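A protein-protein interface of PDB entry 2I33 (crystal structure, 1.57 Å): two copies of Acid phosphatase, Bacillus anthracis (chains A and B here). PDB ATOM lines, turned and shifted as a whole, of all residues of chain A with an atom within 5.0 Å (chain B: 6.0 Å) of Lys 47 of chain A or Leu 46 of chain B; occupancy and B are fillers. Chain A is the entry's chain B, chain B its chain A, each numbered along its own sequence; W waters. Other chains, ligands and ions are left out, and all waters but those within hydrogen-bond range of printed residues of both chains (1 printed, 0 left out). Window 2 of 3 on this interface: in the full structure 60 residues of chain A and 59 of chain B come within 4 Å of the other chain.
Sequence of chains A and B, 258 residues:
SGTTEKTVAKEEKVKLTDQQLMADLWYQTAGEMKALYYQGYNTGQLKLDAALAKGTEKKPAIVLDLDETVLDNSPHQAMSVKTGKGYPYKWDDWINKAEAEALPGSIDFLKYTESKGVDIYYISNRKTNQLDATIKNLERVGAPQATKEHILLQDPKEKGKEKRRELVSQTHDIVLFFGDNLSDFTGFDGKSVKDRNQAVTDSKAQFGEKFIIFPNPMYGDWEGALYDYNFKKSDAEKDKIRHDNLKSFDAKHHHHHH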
ATOM      1  N   THR A  43      15.906 -12.945  -3.351  1.00  0.00           N
ATOM      2  CA  THR A  43      16.989 -13.588  -4.090  1.00  0.00           C
ATOM      3  C   THR A  43      16.536 -14.964  -4.541  1.00  0.00           C
ATOM      4  O   THR A  43      16.764 -15.383  -5.665  1.00  0.00           O
ATOM      5  CB  THR A  43      18.257 -13.668  -3.225  1.00  0.00           C
ATOM      6  OG1 THR A  43      18.589 -12.331  -2.811  1.00  0.00           O
ATOM      7  CG2 THR A  43      19.419 -14.284  -4.016  1.00  0.00           C
ATOM      8  N   GLY A  44      15.844 -15.658  -3.650  1.00  0.00           N
ATOM      9  CA  GLY A  44      15.233 -16.943  -4.005  1.00  0.00           C
ATOM     10  C   GLY A  44      14.357 -16.873  -5.240  1.00  0.00           C
ATOM     11  O   GLY A  44      14.454 -17.705  -6.144  1.00  0.00           O
ATOM     12  N   GLN A  45      13.486 -15.884  -5.303  1.00  0.00           N
ATOM     13  CA  GLN A  45      12.625 -15.721  -6.452  1.00  0.00           C
ATOM     14  C   GLN A  45      13.417 -15.452  -7.727  1.00  0.00           C
ATOM     15  O   GLN A  45      13.139 -16.021  -8.789  1.00  0.00           O
ATOM     16  CB  GLN A  45      11.705 -14.578  -6.186  1.00  0.00           C
ATOM     17  CG  GLN A  45      10.614 -14.518  -7.137  1.00  0.00           C
ATOM     18  CD  GLN A  45       9.442 -13.806  -6.539  1.00  0.00           C
ATOM     19  OE1 GLN A  45       9.146 -13.919  -5.333  1.00  0.00           O
ATOM     20  NE2 GLN A  45       8.776 -13.074  -7.352  1.00  0.00           N
ATOM     21  N   LEU A  46      14.416 -14.592  -7.623  1.00  0.00           N
ATOM     22  CA  LEU A  46      15.239 -14.267  -8.787  1.00  0.00           C
ATOM     23  C   LEU A  46      15.886 -15.548  -9.327  1.00  0.00           C
ATOM     24  O   LEU A  46      15.906 -15.835 -10.534  1.00  0.00           O
ATOM     25  CB  LEU A  46      16.323 -13.271  -8.378  1.00  0.00           C
ATOM     26  CG  LEU A  46      17.251 -12.749  -9.472  1.00  0.00           C
ATOM     27  CD1 LEU A  46      16.533 -11.813 -10.376  1.00  0.00           C
ATOM     28  CD2 LEU A  46      18.445 -12.067  -8.822  1.00  0.00           C
ATOM     29  N   LYS A  47      16.454 -16.304  -8.401  1.00  0.00           N
ATOM     30  CA  LYS A  47      17.170 -17.496  -8.785  1.00  0.00           C
ATOM     31  C   LYS A  47      16.215 -18.572  -9.257  1.00  0.00           C
ATOM     32  O   LYS A  47      16.547 -19.307 -10.177  1.00  0.00           O
ATOM     33  CB  LYS A  47      18.033 -17.995  -7.639  1.00  0.00           C
ATOM     34  CG  LYS A  47      19.140 -16.990  -7.264  1.00  0.00           C
ATOM     35  CD  LYS A  47      20.175 -16.872  -8.354  1.00  0.00           C
ATOM     36  CE  LYS A  47      21.266 -15.834  -8.075  1.00  0.00           C
ATOM     37  NZ  LYS A  47      22.219 -15.743  -9.223  1.00  0.00           N
ATOM     38  N   LEU A  48      15.020 -18.630  -8.691  1.00  0.00           N
ATOM     39  CA  LEU A  48      14.033 -19.612  -9.177  1.00  0.00           C
ATOM     40  C   LEU A  48      13.660 -19.292 -10.620  1.00  0.00           C
ATOM     41  O   LEU A  48      13.627 -20.162 -11.478  1.00  0.00           O
ATOM     42  CB  LEU A  48      12.771 -19.587  -8.320  1.00  0.00           C
ATOM     43  CG  LEU A  48      11.706 -20.596  -8.753  1.00  0.00           C
ATOM     44  CD1 LEU A  48      12.222 -22.028  -8.554  1.00  0.00           C
ATOM     45  CD2 LEU A  48      10.367 -20.340  -8.025  1.00  0.00           C
ATOM     46  N   ASP A  49      13.334 -18.030 -10.883  1.00  0.00           N
ATOM     47  CA  ASP A  49      12.964 -17.662 -12.248  1.00  0.00           C
ATOM     48  C   ASP A  49      14.084 -18.010 -13.230  1.00  0.00           C
ATOM     49  O   ASP A  49      13.819 -18.461 -14.358  1.00  0.00           O
ATOM     50  CB  ASP A  49      12.669 -16.176 -12.347  1.00  0.00           C
ATOM     51  CG  ASP A  49      11.327 -15.811 -11.753  1.00  0.00           C
ATOM     52  OD1 ASP A  49      10.461 -16.710 -11.656  1.00  0.00           O
ATOM     53  OD2 ASP A  49      11.131 -14.625 -11.403  1.00  0.00           O
ATOM     54  N   ALA A  50      15.319 -17.739 -12.826  1.00  0.00           N
ATOM     55  CA  ALA A  50      16.479 -17.976 -13.700  1.00  0.00           C
ATOM     56  C   ALA A  50      16.605 -19.458 -13.977  1.00  0.00           C
ATOM     57  O   ALA A  50      16.891 -19.882 -15.100  1.00  0.00           O
ATOM     58  CB  ALA A  50      17.732 -17.501 -13.041  1.00  0.00           C
ATOM     59  N   ALA A  51      16.381 -20.247 -12.937  1.00  0.00           N
ATOM     60  CA  ALA A  51      16.478 -21.696 -13.072  1.00  0.00           C
ATOM     61  C   ALA A  51      15.399 -22.202 -14.001  1.00  0.00           C
ATOM     62  O   ALA A  51      15.648 -23.059 -14.850  1.00  0.00           O
ATOM     63  CB  ALA A  51      16.371 -22.372 -11.739  1.00  0.00           C
ATOM     64  N   LEU A  52      14.194 -21.683 -13.844  1.00  0.00           N
ATOM     65  CA  LEU A  52      13.094 -22.088 -14.715  1.00  0.00           C
ATOM     66  C   LEU A  52      13.293 -21.659 -16.165  1.00  0.00           C
ATOM     67  O   LEU A  52      12.871 -22.358 -17.076  1.00  0.00           O
ATOM     68  CB  LEU A  52      11.775 -21.537 -14.180  1.00  0.00           C
ATOM     69  CG  LEU A  52      11.372 -22.067 -12.815  1.00  0.00           C
ATOM     70  CD1 LEU A  52      10.125 -21.358 -12.338  1.00  0.00           C
ATOM     71  CD2 LEU A  52      11.197 -23.582 -12.835  1.00  0.00           C
ATOM     72  N   LEU A 176      16.824 -24.881  -5.566  1.00  0.00           N
ATOM     73  CA  LEU A 176      17.177 -24.035  -4.432  1.00  0.00           C
ATOM     74  C   LEU A 176      16.921 -24.715  -3.107  1.00  0.00           C
ATOM     75  O   LEU A 176      15.984 -25.522  -2.998  1.00  0.00           O
ATOM     76  CB  LEU A 176      16.341 -22.761  -4.429  1.00  0.00           C
ATOM     77  CG  LEU A 176      16.519 -21.788  -5.597  1.00  0.00           C
ATOM     78  CD1 LEU A 176      15.363 -20.833  -5.620  1.00  0.00           C
ATOM     79  CD2 LEU A 176      17.828 -21.042  -5.457  1.00  0.00           C
ATOM     80  N   GLY A 208      23.361 -17.580  -1.914  1.00  0.00           N
ATOM     81  CA  GLY A 208      22.631 -16.611  -2.734  1.00  0.00           C
ATOM     82  C   GLY A 208      22.407 -17.107  -4.143  1.00  0.00           C
ATOM     83  O   GLY A 208      21.803 -16.405  -4.950  1.00  0.00           O
ATOM     84  N   GLU A 209      22.842 -18.325  -4.426  1.00  0.00           N
ATOM     85  CA  GLU A 209      22.763 -18.889  -5.774  1.00  0.00           C
ATOM     86  C   GLU A 209      21.903 -20.149  -5.714  1.00  0.00           C
ATOM     87  O   GLU A 209      20.809 -20.190  -6.281  1.00  0.00           O
ATOM     88  CB  GLU A 209      24.167 -19.203  -6.317  1.00  0.00           C
ATOM     89  CG  GLU A 209      24.196 -19.944  -7.629  1.00  0.00           C
ATOM     90  CD  GLU A 209      23.600 -19.165  -8.809  1.00  0.00           C
ATOM     91  OE1 GLU A 209      23.611 -17.915  -8.782  1.00  0.00           O
ATOM     92  OE2 GLU A 209      23.165 -19.821  -9.793  1.00  0.00           O
ATOM     93  N   TYR B  41      27.350 -10.379  -0.492  1.00  0.00           N
ATOM     94  CA  TYR B  41      28.305  -9.910  -1.496  1.00  0.00           C
ATOM     95  C   TYR B  41      28.111 -10.572  -2.847  1.00  0.00           C
ATOM     96  O   TYR B  41      28.298  -9.920  -3.895  1.00  0.00           O
ATOM     97  CB  TYR B  41      29.742  -9.973  -0.980  1.00  0.00           C
ATOM     98  CG  TYR B  41      30.040  -8.844  -0.010  1.00  0.00           C
ATOM     99  CD1 TYR B  41      30.013  -7.512  -0.430  1.00  0.00           C
ATOM    100  CD2 TYR B  41      30.292  -9.103   1.344  1.00  0.00           C
ATOM    101  CE1 TYR B  41      30.263  -6.502   0.447  1.00  0.00           C
ATOM    102  CE2 TYR B  41      30.549  -8.072   2.234  1.00  0.00           C
ATOM    103  CZ  TYR B  41      30.510  -6.779   1.780  1.00  0.00           C
ATOM    104  OH  TYR B  41      30.752  -5.725   2.627  1.00  0.00           O
ATOM    105  N   ASN B  42      27.697 -11.841  -2.867  1.00  0.00           N
ATOM    106  CA  ASN B  42      27.390 -12.455  -4.145  1.00  0.00           C
ATOM    107  C   ASN B  42      26.214 -11.773  -4.832  1.00  0.00           C
ATOM    108  O   ASN B  42      26.218 -11.557  -6.042  1.00  0.00           O
ATOM    109  CB  ASN B  42      27.081 -13.932  -3.978  1.00  0.00           C
ATOM    110  CG  ASN B  42      28.298 -14.742  -3.618  1.00  0.00           C
ATOM    111  OD1 ASN B  42      29.451 -14.306  -3.808  1.00  0.00           O
ATOM    112  ND2 ASN B  42      28.056 -15.931  -3.098  1.00  0.00           N
ATOM    113  N   THR B  43      25.186 -11.495  -4.038  1.00  0.00           N
ATOM    114  CA  THR B  43      23.991 -10.887  -4.555  1.00  0.00           C
ATOM    115  C   THR B  43      24.353  -9.479  -5.005  1.00  0.00           C
ATOM    116  O   THR B  43      23.925  -9.017  -6.061  1.00  0.00           O
ATOM    117  CB  THR B  43      22.898 -10.878  -3.496  1.00  0.00           C
ATOM    118  OG1 THR B  43      22.630 -12.239  -3.119  1.00  0.00           O
ATOM    119  CG2 THR B  43      21.651 -10.221  -4.016  1.00  0.00           C
ATOM    120  N   GLY B  44      25.156  -8.794  -4.214  1.00  0.00           N
ATOM    121  CA  GLY B  44      25.600  -7.461  -4.599  1.00  0.00           C
ATOM    122  C   GLY B  44      26.347  -7.475  -5.935  1.00  0.00           C
ATOM    123  O   GLY B  44      26.166  -6.597  -6.797  1.00  0.00           O
ATOM    124  N   GLN B  45      27.202  -8.462  -6.150  1.00  0.00           N
ATOM    125  CA  GLN B  45      27.918  -8.537  -7.416  1.00  0.00           C
ATOM    126  C   GLN B  45      26.982  -8.740  -8.615  1.00  0.00           C
ATOM    127  O   GLN B  45      27.122  -8.105  -9.657  1.00  0.00           O
ATOM    128  CB  GLN B  45      28.989  -9.612  -7.368  1.00  0.00           C
ATOM    129  CG  GLN B  45      29.884  -9.539  -8.566  1.00  0.00           C
ATOM    130  CD  GLN B  45      31.225 -10.181  -8.341  1.00  0.00           C
ATOM    131  OE1 GLN B  45      31.793 -10.094  -7.240  1.00  0.00           O
ATOM    132  NE2 GLN B  45      31.766 -10.781  -9.389  1.00  0.00           N
ATOM    133  N   LEU B  46      26.008  -9.624  -8.446  1.00  0.00           N
ATOM    134  CA  LEU B  46      25.013  -9.893  -9.469  1.00  0.00           C
ATOM    135  C   LEU B  46      24.261  -8.620  -9.793  1.00  0.00           C
ATOM    136  O   LEU B  46      24.070  -8.274 -10.946  1.00  0.00           O
ATOM    137  CB  LEU B  46      24.028 -10.921  -8.948  1.00  0.00           C
ATOM    138  CG  LEU B  46      22.861 -11.282  -9.858  1.00  0.00           C
ATOM    139  CD1 LEU B  46      23.311 -12.220 -10.919  1.00  0.00           C
ATOM    140  CD2 LEU B  46      21.778 -11.941  -8.992  1.00  0.00           C
ATOM    141  N   LYS B  47      23.849  -7.907  -8.752  1.00  0.00           N
ATOM    142  CA  LYS B  47      23.093  -6.699  -8.957  1.00  0.00           C
ATOM    143  C   LYS B  47      23.962  -5.578  -9.511  1.00  0.00           C
ATOM    144  O   LYS B  47      23.482  -4.743 -10.271  1.00  0.00           O
ATOM    145  CB  LYS B  47      22.408  -6.305  -7.665  1.00  0.00           C
ATOM    146  CG  LYS B  47      21.360  -7.324  -7.219  1.00  0.00           C
ATOM    147  CD  LYS B  47      20.168  -7.375  -8.151  1.00  0.00           C
ATOM    148  CE  LYS B  47      19.121  -8.390  -7.729  1.00  0.00           C
ATOM    149  NZ  LYS B  47      18.035  -8.489  -8.726  1.00  0.00           N
ATOM    150  N   LEU B  48      25.244  -5.576  -9.161  1.00  0.00           N
ATOM    151  CA  LEU B  48      26.162  -4.602  -9.750  1.00  0.00           C
ATOM    152  C   LEU B  48      26.241  -4.810 -11.261  1.00  0.00           C
ATOM    153  O   LEU B  48      26.079  -3.895 -12.033  1.00  0.00           O
ATOM    154  CB  LEU B  48      27.549  -4.709  -9.136  1.00  0.00           C
ATOM    155  CG  LEU B  48      28.561  -3.716  -9.691  1.00  0.00           C
ATOM    156  CD1 LEU B  48      28.106  -2.277  -9.486  1.00  0.00           C
ATOM    157  CD2 LEU B  48      29.952  -3.928  -9.095  1.00  0.00           C
ATOM    158  N   ASP B  49      26.458  -6.044 -11.686  1.00  0.00           N
ATOM    159  CA  ASP B  49      26.504  -6.324 -13.113  1.00  0.00           C
ATOM    160  C   ASP B  49      25.222  -5.915 -13.841  1.00  0.00           C
ATOM    161  O   ASP B  49      25.268  -5.372 -14.930  1.00  0.00           O
ATOM    162  CB  ASP B  49      26.733  -7.798 -13.336  1.00  0.00           C
ATOM    163  CG  ASP B  49      28.155  -8.221 -13.039  1.00  0.00           C
ATOM    164  OD1 ASP B  49      29.065  -7.359 -12.972  1.00  0.00           O
ATOM    165  OD2 ASP B  49      28.366  -9.442 -12.934  1.00  0.00           O
ATOM    166  N   ALA B  50      24.091  -6.206 -13.202  1.00  0.00           N
ATOM    167  CA  ALA B  50      22.782  -5.884 -13.767  1.00  0.00           C
ATOM    168  C   ALA B  50      22.662  -4.380 -13.954  1.00  0.00           C
ATOM    169  O   ALA B  50      22.173  -3.915 -14.979  1.00  0.00           O
ATOM    170  CB  ALA B  50      21.692  -6.351 -12.835  1.00  0.00           C
ATOM    171  N   ALA B  51      23.093  -3.643 -12.928  1.00  0.00           N
ATOM    172  CA  ALA B  51      23.019  -2.193 -12.949  1.00  0.00           C
ATOM    173  C   ALA B  51      23.909  -1.606 -14.027  1.00  0.00           C
ATOM    174  O   ALA B  51      23.517  -0.660 -14.710  1.00  0.00           O
ATOM    175  CB  ALA B  51      23.416  -1.637 -11.621  1.00  0.00           C
HETATM  176  O   HOH W   1      22.731 -13.958  -5.306  1.00  0.00           O
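The side-chain amino group (NZ) of Lys 47 of chain A lies within salt-bridge range of the side-chain carboxylate (OE1) of Glu 209 of chain A (2.6 Å).
Among the printed residues, merely in contact across the chains: Leu 46 of chain A with Leu 46 of chain B, Leu 46 of chain A with Lys 47 of chain B, Lys 47 of chain A with Leu 46 of chain B and Thr 43 of chain A with Thr 43 of chain B.
Of the printed residues of chain B, Leu 46 of chain A touches Leu 46 (3.3 Å) and Lys 47 (3.6 Å).
Of chain B, only Leu 46 (3.8 Å) comes within 4 Å of Lys 47 of chain A.
Gly 208 of chain A touches none of the printed residues of chain B.
Of the printed residues of chain A, Thr 43 of chain B touches Thr 43 (3.9 Å).
Leu 46 of chain B touches two residues of chain A.
Of the printed residues of chain A, Lys 47 of chain B touches Leu 46.
Of the 11 printed residues of chain B, 3 touch a printed residue of chain A.
Of the 13 printed residues of chain A, 3 touch a printed residue of chain B.
Along chain A the printed residues that touch a printed residue of chain B span positions 43 to 47.
Among the printed residues, no Asp or Glu carboxylate lies within 4 Å of a Lys or Arg side-chain nitrogen of the other chain.
Thr 43 of chain B touches its own counterpart, Thr 43 of chain A.
Leu 46 of chain A touches its own counterpart, Leu 46 of chain B.
Leu 46 of chain A touches Lys 47 of chain B, and with the chains exchanged Lys 47 of chain A touches Leu 46 of chain B.
Positions printed for both chains: 43, 44, 45, 46, 47, 48, 49, 50 and 51.
Water W1 lies within hydrogen-bond range of O of Gly 208 of chain A (2.6 Å) and OG1 of Thr 43 of chain B (2.8 Å).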
